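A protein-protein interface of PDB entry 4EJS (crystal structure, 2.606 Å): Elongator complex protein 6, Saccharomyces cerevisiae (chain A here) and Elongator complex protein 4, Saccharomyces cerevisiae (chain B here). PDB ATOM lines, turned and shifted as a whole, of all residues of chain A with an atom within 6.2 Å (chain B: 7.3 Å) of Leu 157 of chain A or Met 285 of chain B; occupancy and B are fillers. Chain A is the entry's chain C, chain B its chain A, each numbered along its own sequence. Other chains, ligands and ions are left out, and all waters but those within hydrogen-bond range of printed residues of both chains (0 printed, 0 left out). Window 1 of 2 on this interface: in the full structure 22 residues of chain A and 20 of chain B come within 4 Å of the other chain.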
ATOM      1  N   PHE A  86     -22.620   3.851   7.146  1.00  0.00           N
ATOM      2  CA  PHE A  86     -23.626   2.985   6.559  1.00  0.00           C
ATOM      3  C   PHE A  86     -23.307   2.563   5.124  1.00  0.00           C
ATOM      4  O   PHE A  86     -24.082   1.825   4.512  1.00  0.00           O
ATOM      5  CB  PHE A  86     -24.992   3.665   6.623  1.00  0.00           C
ATOM      6  CG  PHE A  86     -25.488   3.854   8.021  1.00  0.00           C
ATOM      7  CD1 PHE A  86     -26.345   2.923   8.598  1.00  0.00           C
ATOM      8  CD2 PHE A  86     -25.065   4.946   8.780  1.00  0.00           C
ATOM      9  CE1 PHE A  86     -26.781   3.082   9.914  1.00  0.00           C
ATOM     10  CE2 PHE A  86     -25.499   5.116  10.088  1.00  0.00           C
ATOM     11  CZ  PHE A  86     -26.361   4.191  10.657  1.00  0.00           C
ATOM     12  N   ILE A  87     -22.172   3.021   4.589  1.00  0.00           N
ATOM     13  CA  ILE A  87     -21.826   2.795   3.177  1.00  0.00           C
ATOM     14  C   ILE A  87     -20.439   2.133   2.980  1.00  0.00           C
ATOM     15  O   ILE A  87     -20.202   1.469   1.976  1.00  0.00           O
ATOM     16  CB  ILE A  87     -22.007   4.132   2.319  1.00  0.00           C
ATOM     17  CG1 ILE A  87     -21.975   3.871   0.817  1.00  0.00           C
ATOM     18  CG2 ILE A  87     -21.002   5.203   2.687  1.00  0.00           C
ATOM     19  CD1 ILE A  87     -23.205   3.113   0.310  1.00  0.00           C
ATOM     20  N   GLU A 153     -21.066   8.441   8.838  1.00  0.00           N
ATOM     21  CA  GLU A 153     -21.156   8.602   7.393  1.00  0.00           C
ATOM     22  C   GLU A 153     -22.468   8.030   6.805  1.00  0.00           C
ATOM     23  O   GLU A 153     -22.806   6.858   6.999  1.00  0.00           O
ATOM     24  CB  GLU A 153     -19.927   8.014   6.715  1.00  0.00           C
ATOM     25  CG  GLU A 153     -19.696   8.536   5.326  1.00  0.00           C
ATOM     26  CD  GLU A 153     -18.669   7.724   4.597  1.00  0.00           C
ATOM     27  OE1 GLU A 153     -18.515   6.545   4.981  1.00  0.00           O
ATOM     28  OE2 GLU A 153     -18.027   8.255   3.653  1.00  0.00           O
ATOM     29  N   GLN A 154     -23.210   8.902   6.125  1.00  0.00           N
ATOM     30  CA  GLN A 154     -24.449   8.564   5.406  1.00  0.00           C
ATOM     31  C   GLN A 154     -25.637   7.981   6.193  1.00  0.00           C
ATOM     32  O   GLN A 154     -26.284   7.046   5.726  1.00  0.00           O
ATOM     33  CB  GLN A 154     -24.145   7.706   4.169  1.00  0.00           C
ATOM     34  CG  GLN A 154     -23.363   8.473   3.093  1.00  0.00           C
ATOM     35  CD  GLN A 154     -23.546   7.895   1.703  1.00  0.00           C
ATOM     36  OE1 GLN A 154     -24.617   7.398   1.375  1.00  0.00           O
ATOM     37  NE2 GLN A 154     -22.498   7.951   0.881  1.00  0.00           N
ATOM     38  N   PRO A 155     -25.958   8.561   7.360  1.00  0.00           N
ATOM     39  CA  PRO A 155     -27.156   8.076   8.064  1.00  0.00           C
ATOM     40  C   PRO A 155     -28.456   8.207   7.239  1.00  0.00           C
ATOM     41  O   PRO A 155     -29.371   7.434   7.501  1.00  0.00           O
ATOM     42  CB  PRO A 155     -27.201   8.935   9.341  1.00  0.00           C
ATOM     43  CG  PRO A 155     -26.377  10.201   8.991  1.00  0.00           C
ATOM     44  CD  PRO A 155     -25.313   9.703   8.041  1.00  0.00           C
ATOM     45  N   GLU A 156     -28.526   9.134   6.278  1.00  0.00           N
ATOM     46  CA  GLU A 156     -29.678   9.254   5.357  1.00  0.00           C
ATOM     47  C   GLU A 156     -30.078   7.918   4.733  1.00  0.00           C
ATOM     48  O   GLU A 156     -31.246   7.711   4.425  1.00  0.00           O
ATOM     49  CB  GLU A 156     -29.420  10.212   4.161  1.00  0.00           C
ATOM     50  CG  GLU A 156     -28.428  11.288   4.350  1.00  0.00           C
ATOM     51  CD  GLU A 156     -27.003  10.817   4.197  1.00  0.00           C
ATOM     52  OE1 GLU A 156     -26.592  10.485   3.054  1.00  0.00           O
ATOM     53  OE2 GLU A 156     -26.299  10.799   5.233  1.00  0.00           O
ATOM     54  N   LEU A 157     -29.101   7.051   4.469  1.00  0.00           N
ATOM     55  CA  LEU A 157     -29.396   5.715   3.940  1.00  0.00           C
ATOM     56  C   LEU A 157     -30.521   4.993   4.682  1.00  0.00           C
ATOM     57  O   LEU A 157     -31.262   4.228   4.083  1.00  0.00           O
ATOM     58  CB  LEU A 157     -28.142   4.834   3.906  1.00  0.00           C
ATOM     59  CG  LEU A 157     -27.292   5.133   2.677  1.00  0.00           C
ATOM     60  CD1 LEU A 157     -26.050   4.285   2.664  1.00  0.00           C
ATOM     61  CD2 LEU A 157     -28.143   4.893   1.434  1.00  0.00           C
ATOM     62  N   LEU A 158     -30.634   5.227   5.982  1.00  0.00           N
ATOM     63  CA  LEU A 158     -31.722   4.659   6.766  1.00  0.00           C
ATOM     64  C   LEU A 158     -33.106   5.065   6.245  1.00  0.00           C
ATOM     65  O   LEU A 158     -34.065   4.304   6.375  1.00  0.00           O
ATOM     66  CB  LEU A 158     -31.565   5.046   8.233  1.00  0.00           C
ATOM     67  CG  LEU A 158     -30.337   4.478   8.944  1.00  0.00           C
ATOM     68  CD1 LEU A 158     -30.149   5.154  10.286  1.00  0.00           C
ATOM     69  CD2 LEU A 158     -30.529   2.970   9.126  1.00  0.00           C
ATOM     70  N   LEU A 159     -33.209   6.254   5.648  1.00  0.00           N
ATOM     71  CA  LEU A 159     -34.476   6.707   5.075  1.00  0.00           C
ATOM     72  C   LEU A 159     -34.871   5.850   3.868  1.00  0.00           C
ATOM     73  O   LEU A 159     -36.053   5.670   3.598  1.00  0.00           O
ATOM     74  CB  LEU A 159     -34.416   8.193   4.682  1.00  0.00           C
ATOM     75  CG  LEU A 159     -34.259   9.182   5.839  1.00  0.00           C
ATOM     76  CD1 LEU A 159     -34.221  10.649   5.354  1.00  0.00           C
ATOM     77  CD2 LEU A 159     -35.355   8.981   6.864  1.00  0.00           C
ATOM     78  N   SER A 160     -33.871   5.326   3.155  1.00  0.00           N
ATOM     79  CA  SER A 160     -34.090   4.396   2.044  1.00  0.00           C
ATOM     80  C   SER A 160     -34.158   2.929   2.458  1.00  0.00           C
ATOM     81  O   SER A 160     -34.884   2.169   1.835  1.00  0.00           O
ATOM     82  CB  SER A 160     -33.010   4.554   0.980  1.00  0.00           C
ATOM     83  OG  SER A 160     -32.952   5.892   0.520  1.00  0.00           O
ATOM     84  N   LEU A 161     -33.420   2.537   3.502  1.00  0.00           N
ATOM     85  CA  LEU A 161     -33.317   1.125   3.912  1.00  0.00           C
ATOM     86  C   LEU A 161     -34.415   0.683   4.865  1.00  0.00           C
ATOM     87  O   LEU A 161     -34.707  -0.496   4.970  1.00  0.00           O
ATOM     88  CB  LEU A 161     -31.964   0.811   4.576  1.00  0.00           C
ATOM     89  CG  LEU A 161     -30.649   1.075   3.835  1.00  0.00           C
ATOM     90  CD1 LEU A 161     -29.460   0.814   4.758  1.00  0.00           C
ATOM     91  CD2 LEU A 161     -30.556   0.223   2.585  1.00  0.00           C
ATOM     92  N   VAL A 162     -34.984   1.620   5.604  1.00  0.00           N
ATOM     93  CA  VAL A 162     -36.044   1.280   6.545  1.00  0.00           C
ATOM     94  C   VAL A 162     -37.373   1.749   5.977  1.00  0.00           C
ATOM     95  O   VAL A 162     -37.593   2.945   5.743  1.00  0.00           O
ATOM     96  CB  VAL A 162     -35.819   1.900   7.953  1.00  0.00           C
ATOM     97  CG1 VAL A 162     -36.933   1.477   8.899  1.00  0.00           C
ATOM     98  CG2 VAL A 162     -34.475   1.480   8.511  1.00  0.00           C
ATOM     99  N   LEU A 208     -36.198  12.856   2.075  1.00  0.00           N
ATOM    100  CA  LEU A 208     -34.756  12.802   2.086  1.00  0.00           C
ATOM    101  C   LEU A 208     -34.115  14.193   2.197  1.00  0.00           C
ATOM    102  O   LEU A 208     -33.174  14.395   2.961  1.00  0.00           O
ATOM    103  CB  LEU A 208     -34.306  12.149   0.792  1.00  0.00           C
ATOM    104  CG  LEU A 208     -33.312  11.017   0.920  1.00  0.00           C
ATOM    105  CD1 LEU A 208     -33.087  10.423  -0.455  1.00  0.00           C
ATOM    106  CD2 LEU A 208     -32.016  11.536   1.551  1.00  0.00           C
ATOM    107  N   SER B  45     -17.265  -3.029  -7.634  1.00  0.00           N
ATOM    108  CA  SER B  45     -18.421  -3.265  -8.481  1.00  0.00           C
ATOM    109  C   SER B  45     -18.578  -2.165  -9.528  1.00  0.00           C
ATOM    110  O   SER B  45     -18.244  -1.017  -9.266  1.00  0.00           O
ATOM    111  CB  SER B  45     -19.681  -3.371  -7.618  1.00  0.00           C
ATOM    112  OG  SER B  45     -19.928  -2.167  -6.912  1.00  0.00           O
ATOM    113  N   LEU B  47     -21.570  -0.462 -12.225  1.00  0.00           N
ATOM    114  CA  LEU B  47     -22.905  -0.367 -12.753  1.00  0.00           C
ATOM    115  C   LEU B  47     -22.776   0.261 -14.128  1.00  0.00           C
ATOM    116  O   LEU B  47     -22.247   1.364 -14.262  1.00  0.00           O
ATOM    117  CB  LEU B  47     -23.752   0.520 -11.850  1.00  0.00           C
ATOM    118  CG  LEU B  47     -25.114   0.932 -12.399  1.00  0.00           C
ATOM    119  CD1 LEU B  47     -26.043  -0.275 -12.531  1.00  0.00           C
ATOM    120  CD2 LEU B  47     -25.725   2.023 -11.525  1.00  0.00           C
ATOM    121  N   ILE B 245     -35.147  -2.644  -3.168  1.00  0.00           N
ATOM    122  CA  ILE B 245     -34.053  -2.637  -4.145  1.00  0.00           C
ATOM    123  C   ILE B 245     -32.734  -2.117  -3.542  1.00  0.00           C
ATOM    124  O   ILE B 245     -31.667  -2.697  -3.788  1.00  0.00           O
ATOM    125  CB  ILE B 245     -34.415  -1.916  -5.489  1.00  0.00           C
ATOM    126  CG1 ILE B 245     -33.243  -1.983  -6.462  1.00  0.00           C
ATOM    127  CG2 ILE B 245     -34.800  -0.472  -5.265  1.00  0.00           C
ATOM    128  CD1 ILE B 245     -33.024  -3.372  -7.035  1.00  0.00           C
ATOM    129  N   ILE B 246     -32.802  -1.058  -2.735  1.00  0.00           N
ATOM    130  CA  ILE B 246     -31.584  -0.500  -2.141  1.00  0.00           C
ATOM    131  C   ILE B 246     -31.077  -1.405  -1.015  1.00  0.00           C
ATOM    132  O   ILE B 246     -29.872  -1.498  -0.783  1.00  0.00           O
ATOM    133  CB  ILE B 246     -31.758   0.968  -1.606  1.00  0.00           C
ATOM    134  CG1 ILE B 246     -32.292   1.923  -2.693  1.00  0.00           C
ATOM    135  CG2 ILE B 246     -30.447   1.483  -1.066  1.00  0.00           C
ATOM    136  CD1 ILE B 246     -31.500   1.894  -4.015  1.00  0.00           C
ATOM    137  N   GLY B 247     -31.994  -2.064  -0.305  1.00  0.00           N
ATOM    138  CA  GLY B 247     -31.607  -3.090   0.651  1.00  0.00           C
ATOM    139  C   GLY B 247     -30.899  -4.239  -0.062  1.00  0.00           C
ATOM    140  O   GLY B 247     -29.865  -4.734   0.386  1.00  0.00           O
ATOM    141  N   LEU B 248     -31.450  -4.663  -1.194  1.00  0.00           N
ATOM    142  CA  LEU B 248     -30.774  -5.653  -2.012  1.00  0.00           C
ATOM    143  C   LEU B 248     -29.362  -5.201  -2.421  1.00  0.00           C
ATOM    144  O   LEU B 248     -28.412  -5.970  -2.307  1.00  0.00           O
ATOM    145  CB  LEU B 248     -31.614  -5.999  -3.243  1.00  0.00           C
ATOM    146  CG  LEU B 248     -30.905  -6.947  -4.205  1.00  0.00           C
ATOM    147  CD1 LEU B 248     -30.584  -8.287  -3.545  1.00  0.00           C
ATOM    148  CD2 LEU B 248     -31.774  -7.143  -5.403  1.00  0.00           C
ATOM    149  N   MET B 249     -29.228  -3.959  -2.893  1.00  0.00           N
ATOM    150  CA  MET B 249     -27.948  -3.454  -3.396  1.00  0.00           C
ATOM    151  C   MET B 249     -26.919  -3.213  -2.280  1.00  0.00           C
ATOM    152  O   MET B 249     -25.705  -3.407  -2.455  1.00  0.00           O
ATOM    153  CB  MET B 249     -28.148  -2.186  -4.245  1.00  0.00           C
ATOM    154  CG  MET B 249     -28.709  -2.433  -5.662  1.00  0.00           C
ATOM    155  SD  MET B 249     -28.068  -3.936  -6.496  1.00  0.00           S
ATOM    156  CE  MET B 249     -26.296  -3.683  -6.312  1.00  0.00           C
ATOM    157  N   HIS B 250     -27.426  -2.793  -1.133  1.00  0.00           N
ATOM    158  CA  HIS B 250     -26.623  -2.608   0.062  1.00  0.00           C
ATOM    159  C   HIS B 250     -26.073  -3.946   0.518  1.00  0.00           C
ATOM    160  O   HIS B 250     -24.892  -4.057   0.844  1.00  0.00           O
ATOM    161  CB  HIS B 250     -27.505  -2.030   1.162  1.00  0.00           C
ATOM    162  CG  HIS B 250     -26.751  -1.461   2.319  1.00  0.00           C
ATOM    163  ND1 HIS B 250     -26.418  -2.209   3.430  1.00  0.00           N
ATOM    164  CD2 HIS B 250     -26.293  -0.210   2.555  1.00  0.00           C
ATOM    165  CE1 HIS B 250     -25.782  -1.442   4.297  1.00  0.00           C
ATOM    166  NE2 HIS B 250     -25.689  -0.225   3.789  1.00  0.00           N
ATOM    167  N   GLY B 251     -26.950  -4.951   0.549  1.00  0.00           N
ATOM    168  CA  GLY B 251     -26.596  -6.301   0.955  1.00  0.00           C
ATOM    169  C   GLY B 251     -25.613  -6.976   0.005  1.00  0.00           C
ATOM    170  O   GLY B 251     -24.705  -7.668   0.446  1.00  0.00           O
ATOM    171  N   VAL B 252     -25.793  -6.782  -1.300  1.00  0.00           N
ATOM    172  CA  VAL B 252     -24.835  -7.284  -2.281  1.00  0.00           C
ATOM    173  C   VAL B 252     -23.493  -6.567  -2.153  1.00  0.00           C
ATOM    174  O   VAL B 252     -22.441  -7.202  -2.171  1.00  0.00           O
ATOM    175  CB  VAL B 252     -25.342  -7.149  -3.735  1.00  0.00           C
ATOM    176  CG1 VAL B 252     -24.287  -7.662  -4.692  1.00  0.00           C
ATOM    177  CG2 VAL B 252     -26.625  -7.921  -3.940  1.00  0.00           C
ATOM    178  N   ARG B 253     -23.533  -5.246  -2.013  1.00  0.00           N
ATOM    179  CA  ARG B 253     -22.313  -4.469  -1.806  1.00  0.00           C
ATOM    180  C   ARG B 253     -21.565  -4.947  -0.552  1.00  0.00           C
ATOM    181  O   ARG B 253     -20.339  -5.013  -0.533  1.00  0.00           O
ATOM    182  CB  ARG B 253     -22.621  -2.968  -1.718  1.00  0.00           C
ATOM    183  CG  ARG B 253     -21.490  -2.150  -1.102  1.00  0.00           C
ATOM    184  CD  ARG B 253     -21.852  -0.701  -1.016  1.00  0.00           C
ATOM    185  NE  ARG B 253     -20.750   0.103  -0.504  1.00  0.00           N
ATOM    186  CZ  ARG B 253     -19.791   0.619  -1.260  1.00  0.00           C
ATOM    187  NH1 ARG B 253     -19.797   0.417  -2.566  1.00  0.00           N
ATOM    188  NH2 ARG B 253     -18.822   1.323  -0.708  1.00  0.00           N
ATOM    189  N   SER B 254     -22.317  -5.295   0.484  1.00  0.00           N
ATOM    190  CA  SER B 254     -21.752  -5.803   1.725  1.00  0.00           C
ATOM    191  C   SER B 254     -20.957  -7.101   1.532  1.00  0.00           C
ATOM    192  O   SER B 254     -19.932  -7.317   2.188  1.00  0.00           O
ATOM    193  CB  SER B 254     -22.868  -6.033   2.725  1.00  0.00           C
ATOM    194  OG  SER B 254     -22.438  -6.907   3.734  1.00  0.00           O
ATOM    195  N   LYS B 257     -17.608  -6.417  -0.456  1.00  0.00           N
ATOM    196  CA  LYS B 257     -16.548  -5.907   0.435  1.00  0.00           C
ATOM    197  C   LYS B 257     -16.104  -6.963   1.450  1.00  0.00           C
ATOM    198  O   LYS B 257     -14.935  -7.004   1.843  1.00  0.00           O
ATOM    199  CB  LYS B 257     -16.976  -4.644   1.197  1.00  0.00           C
ATOM    200  CG  LYS B 257     -17.398  -3.457   0.354  1.00  0.00           C
ATOM    201  CD  LYS B 257     -16.423  -3.195  -0.759  1.00  0.00           C
ATOM    202  CE  LYS B 257     -16.941  -2.103  -1.669  1.00  0.00           C
ATOM    203  NZ  LYS B 257     -15.847  -1.489  -2.471  1.00  0.00           N
ATOM    204  N   LEU B 265     -18.469  -7.508  -8.848  1.00  0.00           N
ATOM    205  CA  LEU B 265     -19.859  -7.353  -9.279  1.00  0.00           C
ATOM    206  C   LEU B 265     -20.029  -6.466 -10.513  1.00  0.00           C
ATOM    207  O   LEU B 265     -19.509  -5.354 -10.578  1.00  0.00           O
ATOM    208  CB  LEU B 265     -20.735  -6.841  -8.134  1.00  0.00           C
ATOM    209  CG  LEU B 265     -22.104  -6.295  -8.582  1.00  0.00           C
ATOM    210  CD1 LEU B 265     -23.044  -7.406  -9.003  1.00  0.00           C
ATOM    211  CD2 LEU B 265     -22.742  -5.433  -7.519  1.00  0.00           C
ATOM    212  N   LEU B 279     -32.255   6.175  -9.328  1.00  0.00           N
ATOM    213  CA  LEU B 279     -30.978   6.043 -10.002  1.00  0.00           C
ATOM    214  C   LEU B 279     -29.843   6.615  -9.146  1.00  0.00           C
ATOM    215  O   LEU B 279     -28.776   5.998  -9.037  1.00  0.00           O
ATOM    216  CB  LEU B 279     -31.035   6.703 -11.366  1.00  0.00           C
ATOM    217  CG  LEU B 279     -29.795   6.462 -12.211  1.00  0.00           C
ATOM    218  CD1 LEU B 279     -29.414   4.979 -12.247  1.00  0.00           C
ATOM    219  CD2 LEU B 279     -30.049   6.996 -13.590  1.00  0.00           C
ATOM    220  N   VAL B 280     -30.082   7.771  -8.514  1.00  0.00           N
ATOM    221  CA  VAL B 280     -29.112   8.363  -7.573  1.00  0.00           C
ATOM    222  C   VAL B 280     -28.760   7.444  -6.391  1.00  0.00           C
ATOM    223  O   VAL B 280     -27.589   7.232  -6.092  1.00  0.00           O
ATOM    224  CB  VAL B 280     -29.599   9.720  -7.039  1.00  0.00           C
ATOM    225  CG1 VAL B 280     -28.709  10.189  -5.913  1.00  0.00           C
ATOM    226  CG2 VAL B 280     -29.592  10.738  -8.150  1.00  0.00           C
ATOM    227  N   LEU B 281     -29.779   6.894  -5.733  1.00  0.00           N
ATOM    228  CA  LEU B 281     -29.581   5.843  -4.725  1.00  0.00           C
ATOM    229  C   LEU B 281     -28.768   4.644  -5.225  1.00  0.00           C
ATOM    230  O   LEU B 281     -27.767   4.277  -4.616  1.00  0.00           O
ATOM    231  CB  LEU B 281     -30.924   5.394  -4.135  1.00  0.00           C
ATOM    232  CG  LEU B 281     -31.638   6.587  -3.470  1.00  0.00           C
ATOM    233  CD1 LEU B 281     -33.025   6.242  -2.942  1.00  0.00           C
ATOM    234  CD2 LEU B 281     -30.785   7.123  -2.360  1.00  0.00           C
ATOM    235  N   LEU B 282     -29.188   4.051  -6.339  1.00  0.00           N
ATOM    236  CA  LEU B 282     -28.443   2.964  -6.964  1.00  0.00           C
ATOM    237  C   LEU B 282     -26.967   3.267  -7.210  1.00  0.00           C
ATOM    238  O   LEU B 282     -26.108   2.521  -6.752  1.00  0.00           O
ATOM    239  CB  LEU B 282     -29.093   2.551  -8.275  1.00  0.00           C
ATOM    240  CG  LEU B 282     -30.382   1.758  -8.138  1.00  0.00           C
ATOM    241  CD1 LEU B 282     -30.985   1.518  -9.515  1.00  0.00           C
ATOM    242  CD2 LEU B 282     -30.083   0.455  -7.432  1.00  0.00           C
ATOM    243  N   ARG B 283     -26.668   4.338  -7.947  1.00  0.00           N
ATOM    244  CA  ARG B 283     -25.267   4.715  -8.211  1.00  0.00           C
ATOM    245  C   ARG B 283     -24.389   4.744  -6.970  1.00  0.00           C
ATOM    246  O   ARG B 283     -23.203   4.421  -7.046  1.00  0.00           O
ATOM    247  CB  ARG B 283     -25.173   6.089  -8.850  1.00  0.00           C
ATOM    248  CG  ARG B 283     -25.628   6.154 -10.276  1.00  0.00           C
ATOM    249  CD  ARG B 283     -25.641   7.602 -10.728  1.00  0.00           C
ATOM    250  NE  ARG B 283     -26.034   7.677 -12.117  1.00  0.00           N
ATOM    251  CZ  ARG B 283     -26.613   8.728 -12.676  1.00  0.00           C
ATOM    252  NH1 ARG B 283     -26.878   9.805 -11.949  1.00  0.00           N
ATOM    253  NH2 ARG B 283     -26.930   8.691 -13.966  1.00  0.00           N
ATOM    254  N   ASN B 284     -24.964   5.163  -5.842  1.00  0.00           N
ATOM    255  CA  ASN B 284     -24.226   5.287  -4.583  1.00  0.00           C
ATOM    256  C   ASN B 284     -23.758   3.945  -3.966  1.00  0.00           C
ATOM    257  O   ASN B 284     -22.835   3.914  -3.152  1.00  0.00           O
ATOM    258  CB  ASN B 284     -25.064   6.094  -3.607  1.00  0.00           C
ATOM    259  CG  ASN B 284     -24.380   6.314  -2.273  1.00  0.00           C
ATOM    260  OD1 ASN B 284     -23.308   6.923  -2.188  1.00  0.00           O
ATOM    261  ND2 ASN B 284     -25.021   5.854  -1.215  1.00  0.00           N
ATOM    262  N   MET B 285     -24.374   2.840  -4.379  1.00  0.00           N
ATOM    263  CA  MET B 285     -23.982   1.512  -3.904  1.00  0.00           C
ATOM    264  C   MET B 285     -22.812   0.925  -4.702  1.00  0.00           C
ATOM    265  O   MET B 285     -22.211  -0.064  -4.292  1.00  0.00           O
ATOM    266  CB  MET B 285     -25.172   0.537  -3.965  1.00  0.00           C
ATOM    267  CG  MET B 285     -26.403   0.981  -3.200  1.00  0.00           C
ATOM    268  SD  MET B 285     -26.083   1.077  -1.433  1.00  0.00           S
ATOM    269  CE  MET B 285     -26.265   2.819  -1.123  1.00  0.00           C
ATOM    270  N   PHE B 286     -22.501   1.521  -5.846  1.00  0.00           N
ATOM    271  CA  PHE B 286     -21.463   0.986  -6.713  1.00  0.00           C
ATOM    272  C   PHE B 286     -20.178   1.779  -6.606  1.00  0.00           C
ATOM    273  O   PHE B 286     -20.194   2.974  -6.337  1.00  0.00           O
ATOM    274  CB  PHE B 286     -21.939   0.969  -8.156  1.00  0.00           C
ATOM    275  CG  PHE B 286     -22.960  -0.075  -8.426  1.00  0.00           C
ATOM    276  CD1 PHE B 286     -22.587  -1.298  -8.975  1.00  0.00           C
ATOM    277  CD2 PHE B 286     -24.300   0.149  -8.113  1.00  0.00           C
ATOM    278  CE1 PHE B 286     -23.536  -2.285  -9.213  1.00  0.00           C
ATOM    279  CE2 PHE B 286     -25.261  -0.817  -8.360  1.00  0.00           C
ATOM    280  CZ  PHE B 286     -24.879  -2.042  -8.905  1.00  0.00           C
ATOM    281  N   ASP B 287     -19.058   1.103  -6.813  1.00  0.00           N
ATOM    282  CA  ASP B 287     -17.768   1.771  -6.755  1.00  0.00           C
ATOM    283  C   ASP B 287     -17.516   2.605  -8.013  1.00  0.00           C
ATOM    284  O   ASP B 287     -16.978   3.705  -7.936  1.00  0.00           O
ATOM    285  CB  ASP B 287     -16.650   0.754  -6.494  1.00  0.00           C
ATOM    286  CG  ASP B 287     -16.915  -0.093  -5.242  1.00  0.00           C
ATOM    287  OD1 ASP B 287     -16.792   0.440  -4.115  1.00  0.00           O
ATOM    288  OD2 ASP B 287     -17.253  -1.292  -5.383  1.00  0.00           O
ATOM    289  N   SER B 288     -17.925   2.102  -9.172  1.00  0.00           N
ATOM    290  CA  SER B 288     -17.861   2.911 -10.389  1.00  0.00           C
ATOM    291  C   SER B 288     -19.088   2.763 -11.287  1.00  0.00           C
ATOM    292  O   SER B 288     -19.756   1.726 -11.306  1.00  0.00           O
ATOM    293  CB  SER B 288     -16.577   2.648 -11.173  1.00  0.00           C
ATOM    294  OG  SER B 288     -16.243   1.279 -11.134  1.00  0.00           O
ATOM    295  N   VAL B 289     -19.372   3.831 -12.023  1.00  0.00           N
ATOM    296  CA  VAL B 289     -20.579   3.928 -12.820  1.00  0.00           C
ATOM    297  C   VAL B 289     -20.200   4.336 -14.229  1.00  0.00           C
ATOM    298  O   VAL B 289     -19.463   5.287 -14.421  1.00  0.00           O
ATOM    299  CB  VAL B 289     -21.526   4.996 -12.251  1.00  0.00           C
ATOM    300  CG1 VAL B 289     -22.764   5.128 -13.131  1.00  0.00           C
ATOM    301  CG2 VAL B 289     -21.882   4.684 -10.795  1.00  0.00           C
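CD1 of Ile 87 of chain A touches O of Asn 284 of chain B (3.6 Å).
Ile 87 of chain A touches Met 285 of chain B.
Met 285 of chain B touches Leu 157 of chain A (CE to CD2, 3.8 Å).
Leu 281 of chain B touches Ser 160 of chain A (CD1 to OG, 3.5 Å).
Leu 161 of chain A touches Ile 246 of chain B.
CD2 of Leu 161 of chain A touches N of Gly 247 of chain B, 3.96 Å away.
CD1 of Leu 161 of chain A touches CD2 of His 250 of chain B, 3.99 Å away.
The guanidinium group (NH1) of Arg 253 of chain B is in hydrogen-bond range of the backbone carbonyl oxygen (O) of Met 285 of chain B (3.0 Å).
NH1 of Arg 253 of chain B lies within salt-bridge range of OD1 of Asp 287 of chain B, 3.4 Å away.
The backbone NH of Phe 86 of chain A is in hydrogen-bond range of the backbone carbonyl oxygen of Glu 153 of chain A (3.0 Å).
The backbone carbonyl oxygen of Phe 86 of chain A is in hydrogen-bond range of a ring nitrogen (NE2) of His 250 of chain B.
NE of Arg 253 of chain B is in hydrogen-bond range of O of Ile 87 of chain A (2.9 Å).
ND2 of Asn 284 of chain B lies within hydrogen-bond range of OE1 of Gln 154 of chain A, at 3.0 Å.
Hydrophobic or aromatic side chains of chain A within 4 Å of the printed part of chain B: Ile 87, Leu 157 and Leu 161.
Among the printed residues, no Asp or Glu carboxylate lies within 4 Å of a Lys or Arg side-chain nitrogen of the other chain.
Of chain B, only Met 285 (3.8 Å) comes within 4 Å of Leu 157 of chain A.
Met 285 of chain B touches just these residues of chain A: Ile 87 and Leu 157.
Printed residues of chain B within 4 Å of Gln 154 of chain A: Asn 284.
Of the printed residues of chain A, Gly 247 of chain B touches Leu 161 (3.96 Å).
Of the printed residues of chain A, His 250 of chain B touches Phe 86 (2.7 Å) and Leu 161 (3.99 Å).
Of the printed residues of chain B, Ile 87 of chain A touches Arg 253, Asn 284 and Met 285.
Of the printed residues of chain A, Asn 284 of chain B touches Ile 87 (3.6 Å) and Gln 154 (3.0 Å).
Leu 47 of chain B touches none of the printed residues of chain A.
Leu 265 of chain B touches none of the printed residues of chain A.
The nearest residue of chain B that does not touch Leu 157 of chain A is Asn 284 of chain B (4.2 Å).
The nearest printed residue of chain A that does not touch His 250 of chain B is Leu 157 of chain A (4.5 Å).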
